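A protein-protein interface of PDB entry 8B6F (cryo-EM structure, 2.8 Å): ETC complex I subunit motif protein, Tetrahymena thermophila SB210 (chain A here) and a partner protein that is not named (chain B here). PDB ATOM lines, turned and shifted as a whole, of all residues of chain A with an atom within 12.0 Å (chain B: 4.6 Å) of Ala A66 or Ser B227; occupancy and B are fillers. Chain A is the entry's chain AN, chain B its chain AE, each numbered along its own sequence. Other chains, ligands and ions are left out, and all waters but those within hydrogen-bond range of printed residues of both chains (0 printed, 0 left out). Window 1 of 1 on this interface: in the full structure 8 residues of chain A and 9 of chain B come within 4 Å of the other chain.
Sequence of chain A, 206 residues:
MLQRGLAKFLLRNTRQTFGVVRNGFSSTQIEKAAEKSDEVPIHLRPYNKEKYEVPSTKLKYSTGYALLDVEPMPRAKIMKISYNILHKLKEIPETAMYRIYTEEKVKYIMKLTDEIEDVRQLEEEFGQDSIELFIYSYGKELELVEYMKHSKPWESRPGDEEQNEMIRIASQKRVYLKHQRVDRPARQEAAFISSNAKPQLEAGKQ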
ATOM      1  N   LYS A  60       7.051  18.879  17.148  1.00  0.00           N
ATOM      2  CA  LYS A  60       6.413  20.181  17.268  1.00  0.00           C
ATOM      3  C   LYS A  60       6.912  20.902  18.513  1.00  0.00           C
ATOM      4  O   LYS A  60       7.179  20.282  19.545  1.00  0.00           O
ATOM      5  CB  LYS A  60       4.894  20.034  17.329  1.00  0.00           C
ATOM      6  CG  LYS A  60       4.269  19.493  16.054  1.00  0.00           C
ATOM      7  CD  LYS A  60       2.749  19.570  16.099  1.00  0.00           C
ATOM      8  CE  LYS A  60       2.164  18.742  17.232  1.00  0.00           C
ATOM      9  NZ  LYS A  60       2.584  17.317  17.169  1.00  0.00           N
ATOM     10  N   TYR A  61       7.045  22.224  18.408  1.00  0.00           N
ATOM     11  CA  TYR A  61       7.447  23.014  19.565  1.00  0.00           C
ATOM     12  C   TYR A  61       6.339  23.077  20.607  1.00  0.00           C
ATOM     13  O   TYR A  61       6.621  23.158  21.807  1.00  0.00           O
ATOM     14  CB  TYR A  61       7.840  24.419  19.118  1.00  0.00           C
ATOM     15  CG  TYR A  61       8.694  25.166  20.111  1.00  0.00           C
ATOM     16  CD1 TYR A  61       9.993  24.758  20.384  1.00  0.00           C
ATOM     17  CD2 TYR A  61       8.213  26.294  20.756  1.00  0.00           C
ATOM     18  CE1 TYR A  61      10.781  25.444  21.283  1.00  0.00           C
ATOM     19  CE2 TYR A  61       8.992  26.987  21.657  1.00  0.00           C
ATOM     20  CZ  TYR A  61      10.276  26.557  21.916  1.00  0.00           C
ATOM     21  OH  TYR A  61      11.056  27.246  22.812  1.00  0.00           O
ATOM     22  N   SER A  62       5.082  23.041  20.170  1.00  0.00           N
ATOM     23  CA  SER A  62       3.948  23.027  21.079  1.00  0.00           C
ATOM     24  C   SER A  62       2.792  22.308  20.401  1.00  0.00           C
ATOM     25  O   SER A  62       2.726  22.220  19.173  1.00  0.00           O
ATOM     26  CB  SER A  62       3.536  24.443  21.489  1.00  0.00           C
ATOM     27  OG  SER A  62       3.146  25.206  20.362  1.00  0.00           O
ATOM     28  N   THR A  63       1.877  21.791  21.220  1.00  0.00           N
ATOM     29  CA  THR A  63       0.723  21.070  20.698  1.00  0.00           C
ATOM     30  C   THR A  63      -0.366  21.995  20.174  1.00  0.00           C
ATOM     31  O   THR A  63      -1.181  21.564  19.352  1.00  0.00           O
ATOM     32  CB  THR A  63       0.130  20.163  21.778  1.00  0.00           C
ATOM     33  OG1 THR A  63      -0.158  20.933  22.949  1.00  0.00           O
ATOM     34  CG2 THR A  63       1.095  19.050  22.136  1.00  0.00           C
ATOM     35  N   GLY A  64      -0.401  23.247  20.626  1.00  0.00           N
ATOM     36  CA  GLY A  64      -1.449  24.169  20.258  1.00  0.00           C
ATOM     37  C   GLY A  64      -2.623  24.201  21.212  1.00  0.00           C
ATOM     38  O   GLY A  64      -3.471  25.093  21.093  1.00  0.00           O
ATOM     39  N   TYR A  65      -2.697  23.261  22.148  1.00  0.00           N
ATOM     40  CA  TYR A  65      -3.751  23.212  23.147  1.00  0.00           C
ATOM     41  C   TYR A  65      -3.168  23.516  24.521  1.00  0.00           C
ATOM     42  O   TYR A  65      -2.023  23.167  24.819  1.00  0.00           O
ATOM     43  CB  TYR A  65      -4.432  21.842  23.173  1.00  0.00           C
ATOM     44  CG  TYR A  65      -5.146  21.486  21.893  1.00  0.00           C
ATOM     45  CD1 TYR A  65      -4.469  20.884  20.842  1.00  0.00           C
ATOM     46  CD2 TYR A  65      -6.499  21.742  21.740  1.00  0.00           C
ATOM     47  CE1 TYR A  65      -5.120  20.553  19.672  1.00  0.00           C
ATOM     48  CE2 TYR A  65      -7.159  21.414  20.574  1.00  0.00           C
ATOM     49  CZ  TYR A  65      -6.464  20.820  19.543  1.00  0.00           C
ATOM     50  OH  TYR A  65      -7.118  20.493  18.381  1.00  0.00           O
ATOM     51  N   ALA A  66      -3.967  24.172  25.353  1.00  0.00           N
ATOM     52  CA  ALA A  66      -3.531  24.484  26.704  1.00  0.00           C
ATOM     53  C   ALA A  66      -3.414  23.213  27.533  1.00  0.00           C
ATOM     54  O   ALA A  66      -4.274  22.332  27.476  1.00  0.00           O
ATOM     55  CB  ALA A  66      -4.508  25.452  27.365  1.00  0.00           C
ATOM     56  N   LEU A  67      -2.337  23.125  28.314  1.00  0.00           N
ATOM     57  CA  LEU A  67      -2.126  22.006  29.228  1.00  0.00           C
ATOM     58  C   LEU A  67      -2.135  20.669  28.491  1.00  0.00           C
ATOM     59  O   LEU A  67      -2.710  19.686  28.959  1.00  0.00           O
ATOM     60  CB  LEU A  67      -3.180  22.014  30.333  1.00  0.00           C
ATOM     61  CG  LEU A  67      -3.255  23.304  31.146  1.00  0.00           C
ATOM     62  CD1 LEU A  67      -4.501  23.285  31.985  1.00  0.00           C
ATOM     63  CD2 LEU A  67      -2.024  23.472  32.018  1.00  0.00           C
ATOM     64  N   LEU A  68      -1.496  20.633  27.322  1.00  0.00           N
ATOM     65  CA  LEU A  68      -1.351  19.411  26.529  1.00  0.00           C
ATOM     66  C   LEU A  68       0.108  19.337  26.086  1.00  0.00           C
ATOM     67  O   LEU A  68       0.473  19.863  25.032  1.00  0.00           O
ATOM     68  CB  LEU A  68      -2.311  19.404  25.344  1.00  0.00           C
ATOM     69  CG  LEU A  68      -2.360  18.118  24.513  1.00  0.00           C
ATOM     70  CD1 LEU A  68      -2.880  16.954  25.337  1.00  0.00           C
ATOM     71  CD2 LEU A  68      -3.214  18.312  23.273  1.00  0.00           C
ATOM     72  N   ASP A  69       0.938  18.680  26.894  1.00  0.00           N
ATOM     73  CA  ASP A  69       2.362  18.601  26.615  1.00  0.00           C
ATOM     74  C   ASP A  69       2.630  17.734  25.387  1.00  0.00           C
ATOM     75  O   ASP A  69       1.801  16.923  24.971  1.00  0.00           O
ATOM     76  CB  ASP A  69       3.115  18.037  27.818  1.00  0.00           C
ATOM     77  CG  ASP A  69       3.074  18.961  29.018  1.00  0.00           C
ATOM     78  OD1 ASP A  69       2.453  20.040  28.919  1.00  0.00           O
ATOM     79  OD2 ASP A  69       3.667  18.612  30.060  1.00  0.00           O
ATOM     80  N   VAL A  70       3.814  17.917  24.814  1.00  0.00           N
ATOM     81  CA  VAL A  70       4.205  17.206  23.600  1.00  0.00           C
ATOM     82  C   VAL A  70       4.724  15.826  23.975  1.00  0.00           C
ATOM     83  O   VAL A  70       5.581  15.686  24.854  1.00  0.00           O
ATOM     84  CB  VAL A  70       5.265  18.004  22.823  1.00  0.00           C
ATOM     85  CG1 VAL A  70       5.741  17.225  21.604  1.00  0.00           C
ATOM     86  CG2 VAL A  70       4.716  19.349  22.398  1.00  0.00           C
ATOM     87  N   ASP A 129      -4.404  17.124  13.052  1.00  0.00           N
ATOM     88  CA  ASP A 129      -4.261  17.737  14.361  1.00  0.00           C
ATOM     89  C   ASP A 129      -3.035  17.160  15.067  1.00  0.00           C
ATOM     90  O   ASP A 129      -2.336  16.288  14.547  1.00  0.00           O
ATOM     91  CB  ASP A 129      -5.534  17.522  15.183  1.00  0.00           C
ATOM     92  CG  ASP A 129      -5.712  18.568  16.265  1.00  0.00           C
ATOM     93  OD1 ASP A 129      -4.700  19.148  16.707  1.00  0.00           O
ATOM     94  OD2 ASP A 129      -6.867  18.813  16.673  1.00  0.00           O
ATOM     95  N   SER A 130      -2.775  17.659  16.274  1.00  0.00           N
ATOM     96  CA  SER A 130      -1.634  17.186  17.045  1.00  0.00           C
ATOM     97  C   SER A 130      -1.774  15.701  17.354  1.00  0.00           C
ATOM     98  O   SER A 130      -2.873  15.202  17.611  1.00  0.00           O
ATOM     99  CB  SER A 130      -1.513  17.978  18.347  1.00  0.00           C
ATOM    100  OG  SER A 130      -1.406  19.367  18.091  1.00  0.00           O
ATOM    101  N   GLU A 132      -0.763  14.356  19.963  1.00  0.00           N
ATOM    102  CA  GLU A 132      -1.060  14.210  21.384  1.00  0.00           C
ATOM    103  C   GLU A 132      -2.557  14.101  21.626  1.00  0.00           C
ATOM    104  O   GLU A 132      -2.999  13.323  22.477  1.00  0.00           O
ATOM    105  CB  GLU A 132      -0.473  15.383  22.166  1.00  0.00           C
ATOM    106  CG  GLU A 132       1.047  15.372  22.257  1.00  0.00           C
ATOM    107  CD  GLU A 132       1.725  15.652  20.932  1.00  0.00           C
ATOM    108  OE1 GLU A 132       1.044  16.133  20.003  1.00  0.00           O
ATOM    109  OE2 GLU A 132       2.940  15.395  20.819  1.00  0.00           O
ATOM    110  N   LEU A 133      -3.356  14.881  20.896  1.00  0.00           N
ATOM    111  CA  LEU A 133      -4.803  14.780  21.038  1.00  0.00           C
ATOM    112  C   LEU A 133      -5.296  13.402  20.619  1.00  0.00           C
ATOM    113  O   LEU A 133      -6.174  12.823  21.269  1.00  0.00           O
ATOM    114  CB  LEU A 133      -5.486  15.871  20.214  1.00  0.00           C
ATOM    115  CG  LEU A 133      -7.009  15.956  20.321  1.00  0.00           C
ATOM    116  CD1 LEU A 133      -7.441  16.229  21.752  1.00  0.00           C
ATOM    117  CD2 LEU A 133      -7.538  17.029  19.388  1.00  0.00           C
ATOM    118  N   TYR A 136      -4.474  10.991  23.394  1.00  0.00           N
ATOM    119  CA  TYR A 136      -5.381  11.134  24.525  1.00  0.00           C
ATOM    120  C   TYR A 136      -6.734  10.500  24.235  1.00  0.00           C
ATOM    121  O   TYR A 136      -7.302   9.810  25.088  1.00  0.00           O
ATOM    122  CB  TYR A 136      -5.542  12.616  24.865  1.00  0.00           C
ATOM    123  CG  TYR A 136      -6.469  12.885  26.023  1.00  0.00           C
ATOM    124  CD1 TYR A 136      -6.030  12.770  27.334  1.00  0.00           C
ATOM    125  CD2 TYR A 136      -7.783  13.270  25.803  1.00  0.00           C
ATOM    126  CE1 TYR A 136      -6.877  13.020  28.393  1.00  0.00           C
ATOM    127  CE2 TYR A 136      -8.637  13.522  26.852  1.00  0.00           C
ATOM    128  CZ  TYR A 136      -8.178  13.396  28.145  1.00  0.00           C
ATOM    129  OH  TYR A 136      -9.029  13.649  29.194  1.00  0.00           O
ATOM    130  N   SER A 137      -7.266  10.719  23.033  1.00  0.00           N
ATOM    131  CA  SER A 137      -8.539  10.114  22.666  1.00  0.00           C
ATOM    132  C   SER A 137      -8.425   8.596  22.597  1.00  0.00           C
ATOM    133  O   SER A 137      -9.347   7.879  22.998  1.00  0.00           O
ATOM    134  CB  SER A 137      -9.022  10.695  21.342  1.00  0.00           C
ATOM    135  OG  SER A 137      -9.266  12.082  21.498  1.00  0.00           O
ATOM    136  N   LYS A 140      -8.657   6.359  25.895  1.00  0.00           N
ATOM    137  CA  LYS A 140      -9.924   6.163  26.586  1.00  0.00           C
ATOM    138  C   LYS A 140     -10.541   4.800  26.312  1.00  0.00           C
ATOM    139  O   LYS A 140     -11.414   4.368  27.072  1.00  0.00           O
ATOM    140  CB  LYS A 140     -10.915   7.257  26.192  1.00  0.00           C
ATOM    141  CG  LYS A 140     -10.427   8.659  26.495  1.00  0.00           C
ATOM    142  CD  LYS A 140     -11.436   9.698  26.055  1.00  0.00           C
ATOM    143  CE  LYS A 140     -10.888  11.101  26.246  1.00  0.00           C
ATOM    144  NZ  LYS A 140     -11.850  12.141  25.791  1.00  0.00           N
ATOM    145  N   TYR B 226      -8.514  26.304  32.305  1.00  0.00           N
ATOM    146  CA  TYR B 226      -9.090  25.007  31.990  1.00  0.00           C
ATOM    147  C   TYR B 226      -8.519  24.478  30.679  1.00  0.00           C
ATOM    148  O   TYR B 226      -8.072  25.235  29.817  1.00  0.00           O
ATOM    149  CB  TYR B 226     -10.625  25.068  31.995  1.00  0.00           C
ATOM    150  CG  TYR B 226     -11.242  26.176  31.184  1.00  0.00           C
ATOM    151  CD1 TYR B 226     -11.233  26.143  29.806  1.00  0.00           C
ATOM    152  CD2 TYR B 226     -11.870  27.242  31.810  1.00  0.00           C
ATOM    153  CE1 TYR B 226     -11.818  27.146  29.064  1.00  0.00           C
ATOM    154  CE2 TYR B 226     -12.459  28.249  31.082  1.00  0.00           C
ATOM    155  CZ  TYR B 226     -12.424  28.197  29.707  1.00  0.00           C
ATOM    156  OH  TYR B 226     -13.001  29.202  28.969  1.00  0.00           O
ATOM    157  N   SER B 227      -8.536  23.156  30.568  1.00  0.00           N
ATOM    158  CA  SER B 227      -8.087  22.365  29.431  1.00  0.00           C
ATOM    159  C   SER B 227      -9.172  22.200  28.369  1.00  0.00           C
ATOM    160  O   SER B 227     -10.327  22.592  28.540  1.00  0.00           O
ATOM    161  CB  SER B 227      -7.620  20.987  29.896  1.00  0.00           C
ATOM    162  OG  SER B 227      -6.814  20.370  28.909  1.00  0.00           O
ATOM    163  N   PHE B 228      -8.763  21.594  27.252  1.00  0.00           N
ATOM    164  CA  PHE B 228      -9.687  21.297  26.161  1.00  0.00           C
ATOM    165  C   PHE B 228     -10.780  20.361  26.663  1.00  0.00           C
ATOM    166  O   PHE B 228     -11.943  20.473  26.263  1.00  0.00           O
ATOM    167  CB  PHE B 228      -8.933  20.723  24.955  1.00  0.00           C
ATOM    168  CG  PHE B 228      -8.412  19.332  25.153  1.00  0.00           C
ATOM    169  CD1 PHE B 228      -7.159  19.114  25.699  1.00  0.00           C
ATOM    170  CD2 PHE B 228      -9.152  18.241  24.730  1.00  0.00           C
ATOM    171  CE1 PHE B 228      -6.672  17.832  25.861  1.00  0.00           C
ATOM    172  CE2 PHE B 228      -8.673  16.958  24.890  1.00  0.00           C
ATOM    173  CZ  PHE B 228      -7.431  16.753  25.454  1.00  0.00           C
ATOM    174  N   GLN B 229     -10.413  19.418  27.533  1.00  0.00           N
ATOM    175  CA  GLN B 229     -11.349  18.409  28.021  1.00  0.00           C
ATOM    176  C   GLN B 229     -12.489  19.081  28.781  1.00  0.00           C
ATOM    177  O   GLN B 229     -13.654  18.705  28.624  1.00  0.00           O
ATOM    178  CB  GLN B 229     -10.635  17.378  28.889  1.00  0.00           C
ATOM    179  CG  GLN B 229     -11.512  16.177  29.223  1.00  0.00           C
ATOM    180  CD  GLN B 229     -11.967  15.426  27.984  1.00  0.00           C
ATOM    181  OE1 GLN B 229     -11.335  15.503  26.932  1.00  0.00           O
ATOM    182  NE2 GLN B 229     -13.077  14.707  28.098  1.00  0.00           N
ATOM    183  N   THR B 230     -12.176  20.092  29.598  1.00  0.00           N
ATOM    184  CA  THR B 230     -13.239  20.860  30.243  1.00  0.00           C
ATOM    185  C   THR B 230     -14.032  21.565  29.159  1.00  0.00           C
ATOM    186  O   THR B 230     -15.264  21.644  29.225  1.00  0.00           O
ATOM    187  CB  THR B 230     -12.662  21.866  31.236  1.00  0.00           C
ATOM    188  OG1 THR B 230     -11.956  21.174  32.271  1.00  0.00           O
ATOM    189  CG2 THR B 230     -13.768  22.715  31.852  1.00  0.00           C
ATOM    190  N   CYS B 231     -13.338  22.086  28.153  1.00  0.00           N
ATOM    191  CA  CYS B 231     -13.990  22.835  27.092  1.00  0.00           C
ATOM    192  C   CYS B 231     -14.977  21.890  26.398  1.00  0.00           C
ATOM    193  O   CYS B 231     -16.119  22.257  26.104  1.00  0.00           O
ATOM    194  CB  CYS B 231     -12.947  23.399  26.102  1.00  0.00           C
ATOM    195  SG  CYS B 231     -12.359  25.170  26.275  1.00  0.00           S
ATOM    196  N   CYS B 244      -8.948  27.649  24.934  1.00  0.00           N
ATOM    197  CA  CYS B 244      -8.268  26.371  25.131  1.00  0.00           C
ATOM    198  C   CYS B 244      -7.467  25.949  23.907  1.00  0.00           C
ATOM    199  O   CYS B 244      -6.772  24.930  23.962  1.00  0.00           O
ATOM    200  CB  CYS B 244      -9.265  25.218  25.434  1.00  0.00           C
ATOM    201  SG  CYS B 244     -10.400  25.265  26.883  1.00  0.00           S
ATOM    202  N   GLN B 272      -2.955  29.673  24.101  1.00  0.00           N
ATOM    203  CA  GLN B 272      -2.402  28.444  24.655  1.00  0.00           C
ATOM    204  C   GLN B 272      -2.622  28.322  26.157  1.00  0.00           C
ATOM    205  O   GLN B 272      -2.276  27.287  26.732  1.00  0.00           O
ATOM    206  CB  GLN B 272      -0.903  28.343  24.362  1.00  0.00           C
ATOM    207  CG  GLN B 272      -0.556  28.178  22.892  1.00  0.00           C
ATOM    208  CD  GLN B 272      -0.589  29.485  22.134  1.00  0.00           C
ATOM    209  OE1 GLN B 272      -1.183  30.463  22.583  1.00  0.00           O
ATOM    210  NE2 GLN B 272       0.065  29.513  20.980  1.00  0.00           N
ATOM    211  N   HIS B 273      -3.166  29.351  26.801  1.00  0.00           N
ATOM    212  CA  HIS B 273      -3.536  29.299  28.209  1.00  0.00           C
ATOM    213  C   HIS B 273      -5.034  29.542  28.317  1.00  0.00           C
ATOM    214  O   HIS B 273      -5.548  30.512  27.754  1.00  0.00           O
ATOM    215  CB  HIS B 273      -2.769  30.344  29.024  1.00  0.00           C
ATOM    216  CG  HIS B 273      -1.316  30.436  28.677  1.00  0.00           C
ATOM    217  ND1 HIS B 273      -0.864  31.002  27.504  1.00  0.00           N
ATOM    218  CD2 HIS B 273      -0.211  30.041  29.353  1.00  0.00           C
ATOM    219  CE1 HIS B 273       0.455  30.948  27.471  1.00  0.00           C
ATOM    220  NE2 HIS B 273       0.877  30.370  28.581  1.00  0.00           N
ATOM    221  N   GLY B 274      -5.729  28.663  29.031  1.00  0.00           N
ATOM    222  CA  GLY B 274      -7.172  28.768  29.139  1.00  0.00           C
ATOM    223  C   GLY B 274      -7.627  29.590  30.326  1.00  0.00           C
ATOM    224  O   GLY B 274      -8.485  29.144  31.091  1.00  0.00           O
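Tyr A65 touches Cys B244. Ala A66 touches Ser B227. Ala A66 touches Gln B272 (CB to O, 3.0 Å). N of Gly B274 touches CB of Ala A66 (3.8 Å). Phe B228 touches Leu A68. Leu A133 touches Phe B228 (CD1 to CE2, 3.4 Å). Tyr A136 touches Phe B228 (CD2 to CZ, 3.5 Å). Tyr A136 touches Gln B229 (CE2 to OE1, 3.3 Å). NZ of Lys A140 touches OE1 of Gln B229, 3.6 Å away.
O of Gly B274 lies within hydrogen-bond range of N of Tyr B226 (3.1 Å). The side-chain sulfur (SG) of Cys B244 is disulfide-bonded to the side-chain sulfur (SG) of Cys B231, at 2.1 Å. O of Tyr A65 lies within hydrogen-bond range of OG1 of Thr A63, 3.5 Å away. OG1 of Thr A63 is in hydrogen-bond range of O of Leu A68. OD2 of Asp A129 lies within hydrogen-bond range of OH of Tyr A65. The side-chain hydroxyl of Ser A137 is in hydrogen-bond range of the backbone carbonyl oxygen of Leu A133 (3.2 Å).
Of the 18 printed residues of chain A, 6 touch a printed residue of chain B. Hydrophobic or aromatic side chains of chain A that line the printed part of chain B: Tyr A65, Ala A66, Leu A68, Leu A133 and Tyr A136. Of the 10 printed residues of chain B, 6 touch a printed residue of chain A. Hydrophobic or aromatic side chains of chain B that line the printed part of chain A: Phe B228. Among the printed residues, no Asp or Glu carboxylate lies within 4 Å of a Lys or Arg side-chain nitrogen of the other chain.
The backbone NH (N) of Ala A66 sits at hydrogen-bond distance from the backbone carbonyl oxygen (O) of Cys B244.
Ala A66 touches just these residues of chain B: Ser B227 (3.5 Å), Cys B244 (3.2 Å), Gln B272 (3.0 Å) and Gly B274 (3.8 Å). Of the printed residues of chain A, Ser B227 touches Ala A66. Phe B228 touches just these residues of chain A: Leu A68 (3.9 Å), Leu A133 (3.4 Å) and Tyr A136 (3.5 Å). No residue of chain A comes within 4 Å of Thr B230. Cys B231 touches none of the printed residues of chain A. Cys B244 touches just these residues of chain A: Tyr A65 (3.6 Å) and Ala A66 (3.2 Å). No residue of chain A comes within 4 Å of His B273. Of chain A, only Ala A66 comes within 4 Å of Gly B274. Of the printed residues of chain B, Leu A133 touches Phe B228 (3.4 Å). Printed residues of chain B within 4 Å of Tyr A136: Phe B228 (3.5 Å) and Gln B229 (3.3 Å). Of the printed residues of chain B, Leu A68 touches Phe B228. Printed residues of chain B within 4 Å of Tyr A65: Cys B244 (3.6 Å). Printed residues of chain A within 4 Å of Gln B229: Tyr A136 and Lys A140. The nearest residue of chain A that does not touch Ser B227 is Leu A67 (4.2 Å). The nearest printed residue of chain B that does not touch Lys A140 is Phe B228 (5.8 Å).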
